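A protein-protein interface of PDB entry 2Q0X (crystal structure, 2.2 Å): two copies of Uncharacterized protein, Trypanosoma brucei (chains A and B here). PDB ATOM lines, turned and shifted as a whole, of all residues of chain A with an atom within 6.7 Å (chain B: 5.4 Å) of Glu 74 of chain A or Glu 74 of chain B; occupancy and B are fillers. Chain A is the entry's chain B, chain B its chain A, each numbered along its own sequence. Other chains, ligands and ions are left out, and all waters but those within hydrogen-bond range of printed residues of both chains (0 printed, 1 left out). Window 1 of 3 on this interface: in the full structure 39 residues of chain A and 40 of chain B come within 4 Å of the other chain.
The side-chain carboxylate of Glu 74 of chain A lies close to the side-chain carboxylate of Glu 74 of chain B (3.0 Å).
NZ of Lys 79 of chain A sits at hydrogen-bond distance from O of Glu 49 of chain B, 3.3 Å away.
The side-chain amino group (NZ) of Lys 79 of chain B sits at hydrogen-bond distance from the backbone carbonyl oxygen (O) of Glu 49 of chain A.
The backbone NH (N) of Leu 51 of chain A lies within hydrogen-bond range of the side-chain carboxylate (OE1) of Glu 74 of chain A (2.9 Å).
The backbone NH of Leu 51 of chain B sits at hydrogen-bond distance from the side-chain carboxylate of Glu 74 of chain B, at 3.0 Å.
Among the printed residues, pairs that only touch across the chains: Gly 78 of chain A with Lys 79 of chain B (3.3 Å), Lys 27 of chain A with Ser 50 of chain B (3.5 Å), Glu 74 of chain A with Pro 29 of chain B (3.7 Å), Ser 50 of chain A with Pro 29 of chain B (3.7 Å), Pro 29 of chain A with Glu 74 of chain B (3.9 Å) and Ser 50 of chain A with Lys 79 of chain B (3.97 Å).
Of the printed residues of chain B, Lys 27 of chain A touches Ser 50 (3.5 Å).
Val 44 of chain A touches none of the printed residues of chain B.
Of the printed residues of chain B, Glu 49 of chain A touches Lys 79.
Of the printed residues of chain B, Ser 50 of chain A touches Pro 29 and Lys 79.
Glu 74 of chain A touches two residues of chain B.
Printed residues of chain A within 4 Å of Ser 50 of chain B: Lys 27.
Of chain A, only Pro 29 and Glu 74 come within 4 Å of Glu 74 of chain B.
Pro 76 of chain B touches none of the printed residues of chain A.
Of the printed residues of chain A, Lys 79 of chain B touches Glu 49 (2.5 Å), Ser 50 (3.97 Å) and Gly 78 (3.3 Å).
The nearest residue of chain A that does not touch Glu 74 of chain B is Lys 79 of chain A (4.5 Å).
Of the 11 printed residues of chain B, 5 touch a printed residue of chain A.
Hydrophobic or aromatic side chains of chain B within 4 Å of the printed part of chain A: Pro 29.
Of the 21 printed residues of chain A, 7 touch a printed residue of chain B.
Printed residues of chain A that touch a printed residue of chain B: Lys 27, Pro 29, Glu 49, Ser 50, Glu 74, Gly 78 and Lys 79.
Hydrophobic or aromatic side chains of chain A that line the printed part of chain B: Pro 29.
Among the printed residues, 9 pairs touch across the chains.
Among the printed residues, no Asp or Glu carboxylate lies within 4 Å of a Lys or Arg side-chain nitrogen of the other chain.
Glu 49 of chain A touches Lys 79 of chain B, and with the chains exchanged Lys 79 of chain A touches Glu 49 of chain B.
Ser 50 of chain A touches Pro 29 of chain B, but with the chains exchanged Pro 29 of chain A does not touch Ser 50 of chain B (4.1 Å).
Ser 50 of chain A touches Lys 79 of chain B, but with the chains exchanged Lys 79 of chain A does not touch Ser 50 of chain B (4.6 Å).
Glu 74 of chain B touches its own counterpart, Glu 74 of chain A.
Positions printed for both chains: 28, 29, 49, 50, 51, 72, 73, 74, 75, 76 and 79.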
ATOM      1  N   TYR A  20       9.708 -17.497  -3.202  1.00  0.00           N
ATOM      2  CA  TYR A  20       8.460 -16.910  -2.685  1.00  0.00           C
ATOM      3  C   TYR A  20       8.531 -15.401  -2.769  1.00  0.00           C
ATOM      4  O   TYR A  20       9.608 -14.799  -2.699  1.00  0.00           O
ATOM      5  CB  TYR A  20       8.123 -17.376  -1.262  1.00  0.00           C
ATOM      6  CG  TYR A  20       9.105 -16.955  -0.216  1.00  0.00           C
ATOM      7  CD1 TYR A  20      10.315 -17.619  -0.075  1.00  0.00           C
ATOM      8  CD2 TYR A  20       8.830 -15.890   0.635  1.00  0.00           C
ATOM      9  CE1 TYR A  20      11.227 -17.235   0.883  1.00  0.00           C
ATOM     10  CE2 TYR A  20       9.740 -15.496   1.595  1.00  0.00           C
ATOM     11  CZ  TYR A  20      10.942 -16.181   1.720  1.00  0.00           C
ATOM     12  OH  TYR A  20      11.863 -15.816   2.682  1.00  0.00           O
ATOM     13  N   LYS A  27      11.613 -11.648  -5.752  1.00  0.00           N
ATOM     14  CA  LYS A  27      11.409 -13.054  -5.474  1.00  0.00           C
ATOM     15  C   LYS A  27      12.613 -13.537  -4.689  1.00  0.00           C
ATOM     16  O   LYS A  27      13.741 -13.136  -4.990  1.00  0.00           O
ATOM     17  CB  LYS A  27      11.306 -13.845  -6.764  1.00  0.00           C
ATOM     18  CG  LYS A  27      10.095 -13.530  -7.604  1.00  0.00           C
ATOM     19  CD  LYS A  27       9.896 -14.601  -8.662  1.00  0.00           C
ATOM     20  CE  LYS A  27       8.734 -14.268  -9.534  1.00  0.00           C
ATOM     21  NZ  LYS A  27       8.416 -15.410 -10.389  1.00  0.00           N
ATOM     22  N   ILE A  28      12.367 -14.383  -3.690  1.00  0.00           N
ATOM     23  CA  ILE A  28      13.412 -14.914  -2.815  1.00  0.00           C
ATOM     24  C   ILE A  28      13.625 -16.413  -3.075  1.00  0.00           C
ATOM     25  O   ILE A  28      12.749 -17.232  -2.806  1.00  0.00           O
ATOM     26  CB  ILE A  28      13.067 -14.724  -1.316  1.00  0.00           C
ATOM     27  CG1 ILE A  28      12.923 -13.236  -0.975  1.00  0.00           C
ATOM     28  CG2 ILE A  28      14.140 -15.365  -0.457  1.00  0.00           C
ATOM     29  CD1 ILE A  28      12.175 -12.950   0.342  1.00  0.00           C
ATOM     30  N   PRO A  29      14.797 -16.777  -3.588  1.00  0.00           N
ATOM     31  CA  PRO A  29      15.015 -18.177  -3.835  1.00  0.00           C
ATOM     32  C   PRO A  29      15.400 -18.968  -2.590  1.00  0.00           C
ATOM     33  O   PRO A  29      16.058 -18.459  -1.673  1.00  0.00           O
ATOM     34  CB  PRO A  29      16.122 -18.191  -4.892  1.00  0.00           C
ATOM     35  CG  PRO A  29      16.849 -16.958  -4.690  1.00  0.00           C
ATOM     36  CD  PRO A  29      15.942 -15.951  -4.015  1.00  0.00           C
ATOM     37  N   VAL A  30      14.928 -20.210  -2.583  1.00  0.00           N
ATOM     38  CA  VAL A  30      15.091 -21.118  -1.480  1.00  0.00           C
ATOM     39  C   VAL A  30      15.523 -22.453  -2.077  1.00  0.00           C
ATOM     40  O   VAL A  30      14.872 -22.959  -2.972  1.00  0.00           O
ATOM     41  CB  VAL A  30      13.771 -21.306  -0.705  1.00  0.00           C
ATOM     42  CG1 VAL A  30      13.992 -22.234   0.476  1.00  0.00           C
ATOM     43  CG2 VAL A  30      13.200 -19.956  -0.225  1.00  0.00           C
ATOM     44  N   PHE A  31      16.608 -23.021  -1.562  1.00  0.00           N
ATOM     45  CA  PHE A  31      17.112 -24.301  -2.037  1.00  0.00           C
ATOM     46  C   PHE A  31      17.001 -25.338  -0.917  1.00  0.00           C
ATOM     47  O   PHE A  31      17.569 -25.174   0.145  1.00  0.00           O
ATOM     48  CB  PHE A  31      18.559 -24.156  -2.585  1.00  0.00           C
ATOM     49  CG  PHE A  31      19.102 -25.415  -3.211  1.00  0.00           C
ATOM     50  CD1 PHE A  31      20.089 -26.155  -2.575  1.00  0.00           C
ATOM     51  CD2 PHE A  31      18.613 -25.870  -4.409  1.00  0.00           C
ATOM     52  CE1 PHE A  31      20.583 -27.318  -3.141  1.00  0.00           C
ATOM     53  CE2 PHE A  31      19.108 -27.033  -4.982  1.00  0.00           C
ATOM     54  CZ  PHE A  31      20.095 -27.757  -4.338  1.00  0.00           C
ATOM     55  N   TRP A  43      19.335 -22.302   6.934  1.00  0.00           N
ATOM     56  CA  TRP A  43      20.478 -21.427   6.936  1.00  0.00           C
ATOM     57  C   TRP A  43      20.167 -20.078   6.333  1.00  0.00           C
ATOM     58  O   TRP A  43      19.602 -19.993   5.235  1.00  0.00           O
ATOM     59  CB  TRP A  43      21.640 -22.051   6.162  1.00  0.00           C
ATOM     60  CG  TRP A  43      22.814 -21.114   6.053  1.00  0.00           C
ATOM     61  CD1 TRP A  43      23.749 -20.873   7.012  1.00  0.00           C
ATOM     62  CD2 TRP A  43      23.155 -20.281   4.935  1.00  0.00           C
ATOM     63  NE1 TRP A  43      24.659 -19.958   6.564  1.00  0.00           N
ATOM     64  CE2 TRP A  43      24.316 -19.564   5.294  1.00  0.00           C
ATOM     65  CE3 TRP A  43      22.590 -20.070   3.668  1.00  0.00           C
ATOM     66  CZ2 TRP A  43      24.950 -18.657   4.420  1.00  0.00           C
ATOM     67  CZ3 TRP A  43      23.199 -19.157   2.806  1.00  0.00           C
ATOM     68  CH2 TRP A  43      24.385 -18.467   3.184  1.00  0.00           C
ATOM     69  N   VAL A  44      20.560 -19.026   7.045  1.00  0.00           N
ATOM     70  CA  VAL A  44      20.629 -17.675   6.477  1.00  0.00           C
ATOM     71  C   VAL A  44      21.981 -17.028   6.841  1.00  0.00           C
ATOM     72  O   VAL A  44      22.570 -17.288   7.909  1.00  0.00           O
ATOM     73  CB  VAL A  44      19.378 -16.804   6.867  1.00  0.00           C
ATOM     74  CG1 VAL A  44      19.359 -16.441   8.336  1.00  0.00           C
ATOM     75  CG2 VAL A  44      19.320 -15.570   5.999  1.00  0.00           C
ATOM     76  N   GLY A  45      22.498 -16.226   5.920  1.00  0.00           N
ATOM     77  CA  GLY A  45      23.851 -15.705   6.035  1.00  0.00           C
ATOM     78  C   GLY A  45      24.002 -14.204   5.924  1.00  0.00           C
ATOM     79  O   GLY A  45      23.031 -13.435   6.008  1.00  0.00           O
ATOM     80  N   GLU A  49      26.942 -13.356   1.296  1.00  0.00           N
ATOM     81  CA  GLU A  49      26.977 -14.830   1.242  1.00  0.00           C
ATOM     82  C   GLU A  49      25.927 -15.374   0.273  1.00  0.00           C
ATOM     83  O   GLU A  49      24.800 -14.875   0.204  1.00  0.00           O
ATOM     84  CB  GLU A  49      26.853 -15.468   2.634  1.00  0.00           C
ATOM     85  CG  GLU A  49      28.090 -15.251   3.489  1.00  0.00           C
ATOM     86  CD  GLU A  49      28.091 -15.926   4.877  1.00  0.00           C
ATOM     87  OE1 GLU A  49      27.060 -15.980   5.572  1.00  0.00           O
ATOM     88  OE2 GLU A  49      29.188 -16.341   5.321  1.00  0.00           O
ATOM     89  N   SER A  50      26.324 -16.398  -0.479  1.00  0.00           N
ATOM     90  CA  SER A  50      25.517 -16.966  -1.540  1.00  0.00           C
ATOM     91  C   SER A  50      25.023 -18.317  -1.075  1.00  0.00           C
ATOM     92  O   SER A  50      25.555 -18.875  -0.139  1.00  0.00           O
ATOM     93  CB  SER A  50      26.375 -17.142  -2.806  1.00  0.00           C
ATOM     94  OG  SER A  50      27.356 -18.203  -2.671  1.00  0.00           O
ATOM     95  N   LEU A  51      24.007 -18.849  -1.741  1.00  0.00           N
ATOM     96  CA  LEU A  51      23.665 -20.247  -1.586  1.00  0.00           C
ATOM     97  C   LEU A  51      24.961 -21.040  -1.672  1.00  0.00           C
ATOM     98  O   LEU A  51      25.834 -20.709  -2.488  1.00  0.00           O
ATOM     99  CB  LEU A  51      22.736 -20.669  -2.707  1.00  0.00           C
ATOM    100  CG  LEU A  51      21.326 -20.074  -2.758  1.00  0.00           C
ATOM    101  CD1 LEU A  51      20.559 -20.601  -3.990  1.00  0.00           C
ATOM    102  CD2 LEU A  51      20.550 -20.335  -1.445  1.00  0.00           C
ATOM    103  N   LEU A  52      25.108 -22.053  -0.820  1.00  0.00           N
ATOM    104  CA  LEU A  52      26.350 -22.825  -0.730  1.00  0.00           C
ATOM    105  C   LEU A  52      27.606 -21.951  -0.477  1.00  0.00           C
ATOM    106  O   LEU A  52      28.700 -22.237  -0.991  1.00  0.00           O
ATOM    107  CB  LEU A  52      26.534 -23.708  -1.974  1.00  0.00           C
ATOM    108  CG  LEU A  52      25.497 -24.806  -2.265  1.00  0.00           C
ATOM    109  CD1 LEU A  52      25.794 -25.439  -3.620  1.00  0.00           C
ATOM    110  CD2 LEU A  52      25.470 -25.864  -1.175  1.00  0.00           C
ATOM    111  N   GLN A  72      18.317 -23.511   2.421  1.00  0.00           N
ATOM    112  CA  GLN A  72      19.098 -22.295   2.329  1.00  0.00           C
ATOM    113  C   GLN A  72      18.282 -21.237   1.659  1.00  0.00           C
ATOM    114  O   GLN A  72      17.621 -21.489   0.667  1.00  0.00           O
ATOM    115  CB  GLN A  72      20.386 -22.518   1.534  1.00  0.00           C
ATOM    116  CG  GLN A  72      21.274 -23.618   2.089  1.00  0.00           C
ATOM    117  CD  GLN A  72      22.420 -23.951   1.154  1.00  0.00           C
ATOM    118  OE1 GLN A  72      23.354 -23.170   1.016  1.00  0.00           O
ATOM    119  NE2 GLN A  72      22.351 -25.119   0.502  1.00  0.00           N
ATOM    120  N   VAL A  73      18.325 -20.047   2.224  1.00  0.00           N
ATOM    121  CA  VAL A  73      17.663 -18.899   1.651  1.00  0.00           C
ATOM    122  C   VAL A  73      18.711 -17.802   1.489  1.00  0.00           C
ATOM    123  O   VAL A  73      19.590 -17.643   2.329  1.00  0.00           O
ATOM    124  CB  VAL A  73      16.458 -18.443   2.521  1.00  0.00           C
ATOM    125  CG1 VAL A  73      16.898 -18.000   3.907  1.00  0.00           C
ATOM    126  CG2 VAL A  73      15.663 -17.336   1.834  1.00  0.00           C
ATOM    127  N   GLU A  74      18.623 -17.068   0.393  1.00  0.00           N
ATOM    128  CA  GLU A  74      19.457 -15.897   0.217  1.00  0.00           C
ATOM    129  C   GLU A  74      18.707 -14.680   0.751  1.00  0.00           C
ATOM    130  O   GLU A  74      17.617 -14.345   0.283  1.00  0.00           O
ATOM    131  CB  GLU A  74      19.896 -15.728  -1.271  1.00  0.00           C
ATOM    132  CG  GLU A  74      21.254 -16.441  -1.572  1.00  0.00           C
ATOM    133  CD  GLU A  74      21.792 -16.212  -2.989  1.00  0.00           C
ATOM    134  OE1 GLU A  74      22.813 -16.829  -3.372  1.00  0.00           O
ATOM    135  OE2 GLU A  74      21.190 -15.418  -3.740  1.00  0.00           O
ATOM    136  N   VAL A  75      19.324 -14.023   1.718  1.00  0.00           N
ATOM    137  CA  VAL A  75      18.761 -12.845   2.378  1.00  0.00           C
ATOM    138  C   VAL A  75      18.421 -11.784   1.356  1.00  0.00           C
ATOM    139  O   VAL A  75      19.275 -11.406   0.575  1.00  0.00           O
ATOM    140  CB  VAL A  75      19.781 -12.210   3.347  1.00  0.00           C
ATOM    141  CG1 VAL A  75      19.106 -11.174   4.190  1.00  0.00           C
ATOM    142  CG2 VAL A  75      20.375 -13.251   4.219  1.00  0.00           C
ATOM    143  N   PRO A  76      17.181 -11.282   1.367  1.00  0.00           N
ATOM    144  CA  PRO A  76      16.778 -10.285   0.369  1.00  0.00           C
ATOM    145  C   PRO A  76      17.681  -9.039   0.296  1.00  0.00           C
ATOM    146  O   PRO A  76      17.956  -8.545  -0.803  1.00  0.00           O
ATOM    147  CB  PRO A  76      15.366  -9.909   0.806  1.00  0.00           C
ATOM    148  CG  PRO A  76      14.912 -11.042   1.609  1.00  0.00           C
ATOM    149  CD  PRO A  76      16.081 -11.620   2.278  1.00  0.00           C
ATOM    150  N   SER A  77      18.141  -8.568   1.457  1.00  0.00           N
ATOM    151  CA  SER A  77      18.999  -7.380   1.560  1.00  0.00           C
ATOM    152  C   SER A  77      20.445  -7.598   1.087  1.00  0.00           C
ATOM    153  O   SER A  77      21.234  -6.652   1.063  1.00  0.00           O
ATOM    154  CB  SER A  77      19.035  -6.878   3.009  1.00  0.00           C
ATOM    155  OG  SER A  77      19.763  -7.780   3.826  1.00  0.00           O
ATOM    156  N   GLY A  78      20.793  -8.833   0.736  1.00  0.00           N
ATOM    157  CA  GLY A  78      22.051  -9.116   0.055  1.00  0.00           C
ATOM    158  C   GLY A  78      22.011  -8.755  -1.431  1.00  0.00           C
ATOM    159  O   GLY A  78      23.028  -8.805  -2.119  1.00  0.00           O
ATOM    160  N   LYS A  79      20.826  -8.395  -1.908  1.00  0.00           N
ATOM    161  CA  LYS A  79      20.578  -8.153  -3.308  1.00  0.00           C
ATOM    162  C   LYS A  79      20.383  -6.656  -3.500  1.00  0.00           C
ATOM    163  O   LYS A  79      19.874  -5.963  -2.616  1.00  0.00           O
ATOM    164  CB  LYS A  79      19.335  -8.948  -3.740  1.00  0.00           C
ATOM    165  CG  LYS A  79      19.160  -9.136  -5.223  1.00  0.00           C
ATOM    166  CD  LYS A  79      20.058 -10.224  -5.823  1.00  0.00           C
ATOM    167  CE  LYS A  79      19.567 -10.562  -7.225  1.00  0.00           C
ATOM    168  NZ  LYS A  79      20.615 -10.907  -8.256  1.00  0.00           N
ATOM    169  N   ILE B  28      29.679 -17.657  -6.967  1.00  0.00           N
ATOM    170  CA  ILE B  28      28.544 -17.460  -7.848  1.00  0.00           C
ATOM    171  C   ILE B  28      27.761 -18.774  -7.945  1.00  0.00           C
ATOM    172  O   ILE B  28      28.297 -19.782  -8.416  1.00  0.00           O
ATOM    173  CB  ILE B  28      29.011 -17.024  -9.254  1.00  0.00           C
ATOM    174  CG1 ILE B  28      29.891 -15.763  -9.162  1.00  0.00           C
ATOM    175  CG2 ILE B  28      27.826 -16.786 -10.146  1.00  0.00           C
ATOM    176  CD1 ILE B  28      30.691 -15.488 -10.416  1.00  0.00           C
ATOM    177  N   PRO B  29      26.510 -18.777  -7.461  1.00  0.00           N
ATOM    178  CA  PRO B  29      25.632 -19.917  -7.628  1.00  0.00           C
ATOM    179  C   PRO B  29      25.098 -20.118  -9.032  1.00  0.00           C
ATOM    180  O   PRO B  29      24.720 -19.162  -9.728  1.00  0.00           O
ATOM    181  CB  PRO B  29      24.454 -19.611  -6.694  1.00  0.00           C
ATOM    182  CG  PRO B  29      24.889 -18.538  -5.843  1.00  0.00           C
ATOM    183  CD  PRO B  29      25.868 -17.739  -6.646  1.00  0.00           C
ATOM    184  N   GLU B  49      16.990  -9.416 -10.575  1.00  0.00           N
ATOM    185  CA  GLU B  49      16.354 -10.664 -10.946  1.00  0.00           C
ATOM    186  C   GLU B  49      17.067 -11.831 -10.252  1.00  0.00           C
ATOM    187  O   GLU B  49      18.293 -11.944 -10.303  1.00  0.00           O
ATOM    188  CB  GLU B  49      16.349 -10.851 -12.471  1.00  0.00           C
ATOM    189  CG  GLU B  49      15.380  -9.902 -13.170  1.00  0.00           C
ATOM    190  CD  GLU B  49      15.278 -10.128 -14.682  1.00  0.00           C
ATOM    191  OE1 GLU B  49      16.317 -10.217 -15.367  1.00  0.00           O
ATOM    192  OE2 GLU B  49      14.139 -10.186 -15.202  1.00  0.00           O
ATOM    193  N   SER B  50      16.272 -12.690  -9.626  1.00  0.00           N
ATOM    194  CA  SER B  50      16.737 -13.853  -8.893  1.00  0.00           C
ATOM    195  C   SER B  50      16.718 -15.093  -9.755  1.00  0.00           C
ATOM    196  O   SER B  50      16.120 -15.101 -10.835  1.00  0.00           O
ATOM    197  CB  SER B  50      15.782 -14.086  -7.700  1.00  0.00           C
ATOM    198  OG  SER B  50      14.480 -14.569  -8.132  1.00  0.00           O
ATOM    199  N   LEU B  51      17.339 -16.159  -9.265  1.00  0.00           N
ATOM    200  CA  LEU B  51      17.109 -17.476  -9.820  1.00  0.00           C
ATOM    201  C   LEU B  51      15.607 -17.687  -9.921  1.00  0.00           C
ATOM    202  O   LEU B  51      14.869 -17.274  -9.020  1.00  0.00           O
ATOM    203  CB  LEU B  51      17.703 -18.575  -8.928  1.00  0.00           C
ATOM    204  CG  LEU B  51      19.219 -18.711  -8.802  1.00  0.00           C
ATOM    205  CD1 LEU B  51      19.560 -19.888  -7.868  1.00  0.00           C
ATOM    206  CD2 LEU B  51      19.905 -18.804 -10.193  1.00  0.00           C
ATOM    207  N   GLN B  72      20.830 -21.466 -14.954  1.00  0.00           N
ATOM    208  CA  GLN B  72      20.608 -20.122 -14.422  1.00  0.00           C
ATOM    209  C   GLN B  72      21.743 -19.716 -13.518  1.00  0.00           C
ATOM    210  O   GLN B  72      22.179 -20.496 -12.687  1.00  0.00           O
ATOM    211  CB  GLN B  72      19.331 -20.108 -13.602  1.00  0.00           C
ATOM    212  CG  GLN B  72      18.103 -20.352 -14.410  1.00  0.00           C
ATOM    213  CD  GLN B  72      16.868 -20.482 -13.538  1.00  0.00           C
ATOM    214  OE1 GLN B  72      16.306 -19.481 -13.083  1.00  0.00           O
ATOM    215  NE2 GLN B  72      16.458 -21.723 -13.277  1.00  0.00           N
ATOM    216  N   VAL B  73      22.214 -18.488 -13.683  1.00  0.00           N
ATOM    217  CA  VAL B  73      23.278 -17.933 -12.850  1.00  0.00           C
ATOM    218  C   VAL B  73      22.770 -16.593 -12.374  1.00  0.00           C
ATOM    219  O   VAL B  73      22.087 -15.880 -13.116  1.00  0.00           O
ATOM    220  CB  VAL B  73      24.641 -17.781 -13.631  1.00  0.00           C
ATOM    221  CG1 VAL B  73      24.538 -16.807 -14.797  1.00  0.00           C
ATOM    222  CG2 VAL B  73      25.810 -17.366 -12.699  1.00  0.00           C
ATOM    223  N   GLU B  74      23.101 -16.237 -11.140  1.00  0.00           N
ATOM    224  CA  GLU B  74      22.844 -14.878 -10.679  1.00  0.00           C
ATOM    225  C   GLU B  74      24.039 -13.993 -10.971  1.00  0.00           C
ATOM    226  O   GLU B  74      25.149 -14.291 -10.553  1.00  0.00           O
ATOM    227  CB  GLU B  74      22.466 -14.865  -9.197  1.00  0.00           C
ATOM    228  CG  GLU B  74      21.028 -15.316  -8.986  1.00  0.00           C
ATOM    229  CD  GLU B  74      20.657 -15.515  -7.513  1.00  0.00           C
ATOM    230  OE1 GLU B  74      19.417 -15.599  -7.240  1.00  0.00           O
ATOM    231  OE2 GLU B  74      21.605 -15.594  -6.659  1.00  0.00           O
ATOM    232  N   VAL B  75      23.790 -12.914 -11.703  1.00  0.00           N
ATOM    233  CA  VAL B  75      24.792 -11.871 -11.981  1.00  0.00           C
ATOM    234  C   VAL B  75      25.451 -11.418 -10.678  1.00  0.00           C
ATOM    235  O   VAL B  75      24.756 -10.976  -9.781  1.00  0.00           O
ATOM    236  CB  VAL B  75      24.144 -10.612 -12.638  1.00  0.00           C
ATOM    237  CG1 VAL B  75      25.209  -9.616 -13.043  1.00  0.00           C
ATOM    238  CG2 VAL B  75      23.388 -10.976 -13.828  1.00  0.00           C
ATOM    239  N   PRO B  76      26.797 -11.518 -10.581  1.00  0.00           N
ATOM    240  CA  PRO B  76      27.525 -11.146  -9.354  1.00  0.00           C
ATOM    241  C   PRO B  76      27.283  -9.707  -8.872  1.00  0.00           C
ATOM    242  O   PRO B  76      27.256  -9.454  -7.669  1.00  0.00           O
ATOM    243  CB  PRO B  76      28.991 -11.312  -9.754  1.00  0.00           C
ATOM    244  CG  PRO B  76      28.975 -12.250 -10.905  1.00  0.00           C
ATOM    245  CD  PRO B  76      27.699 -12.031 -11.625  1.00  0.00           C
ATOM    246  N   LYS B  79      24.628  -8.571  -6.347  1.00  0.00           N
ATOM    247  CA  LYS B  79      24.846  -8.701  -4.917  1.00  0.00           C
ATOM    248  C   LYS B  79      25.604  -7.515  -4.328  1.00  0.00           C
ATOM    249  O   LYS B  79      26.461  -6.903  -4.988  1.00  0.00           O
ATOM    250  CB  LYS B  79      25.588 -10.010  -4.619  1.00  0.00           C
ATOM    251  CG  LYS B  79      24.758 -11.256  -4.937  1.00  0.00           C
ATOM    252  CD  LYS B  79      24.910 -12.369  -3.889  1.00  0.00           C
ATOM    253  CE  LYS B  79      24.266 -12.011  -2.557  1.00  0.00           C
ATOM    254  NZ  LYS B  79      24.359 -13.120  -1.567  1.00  0.00           N
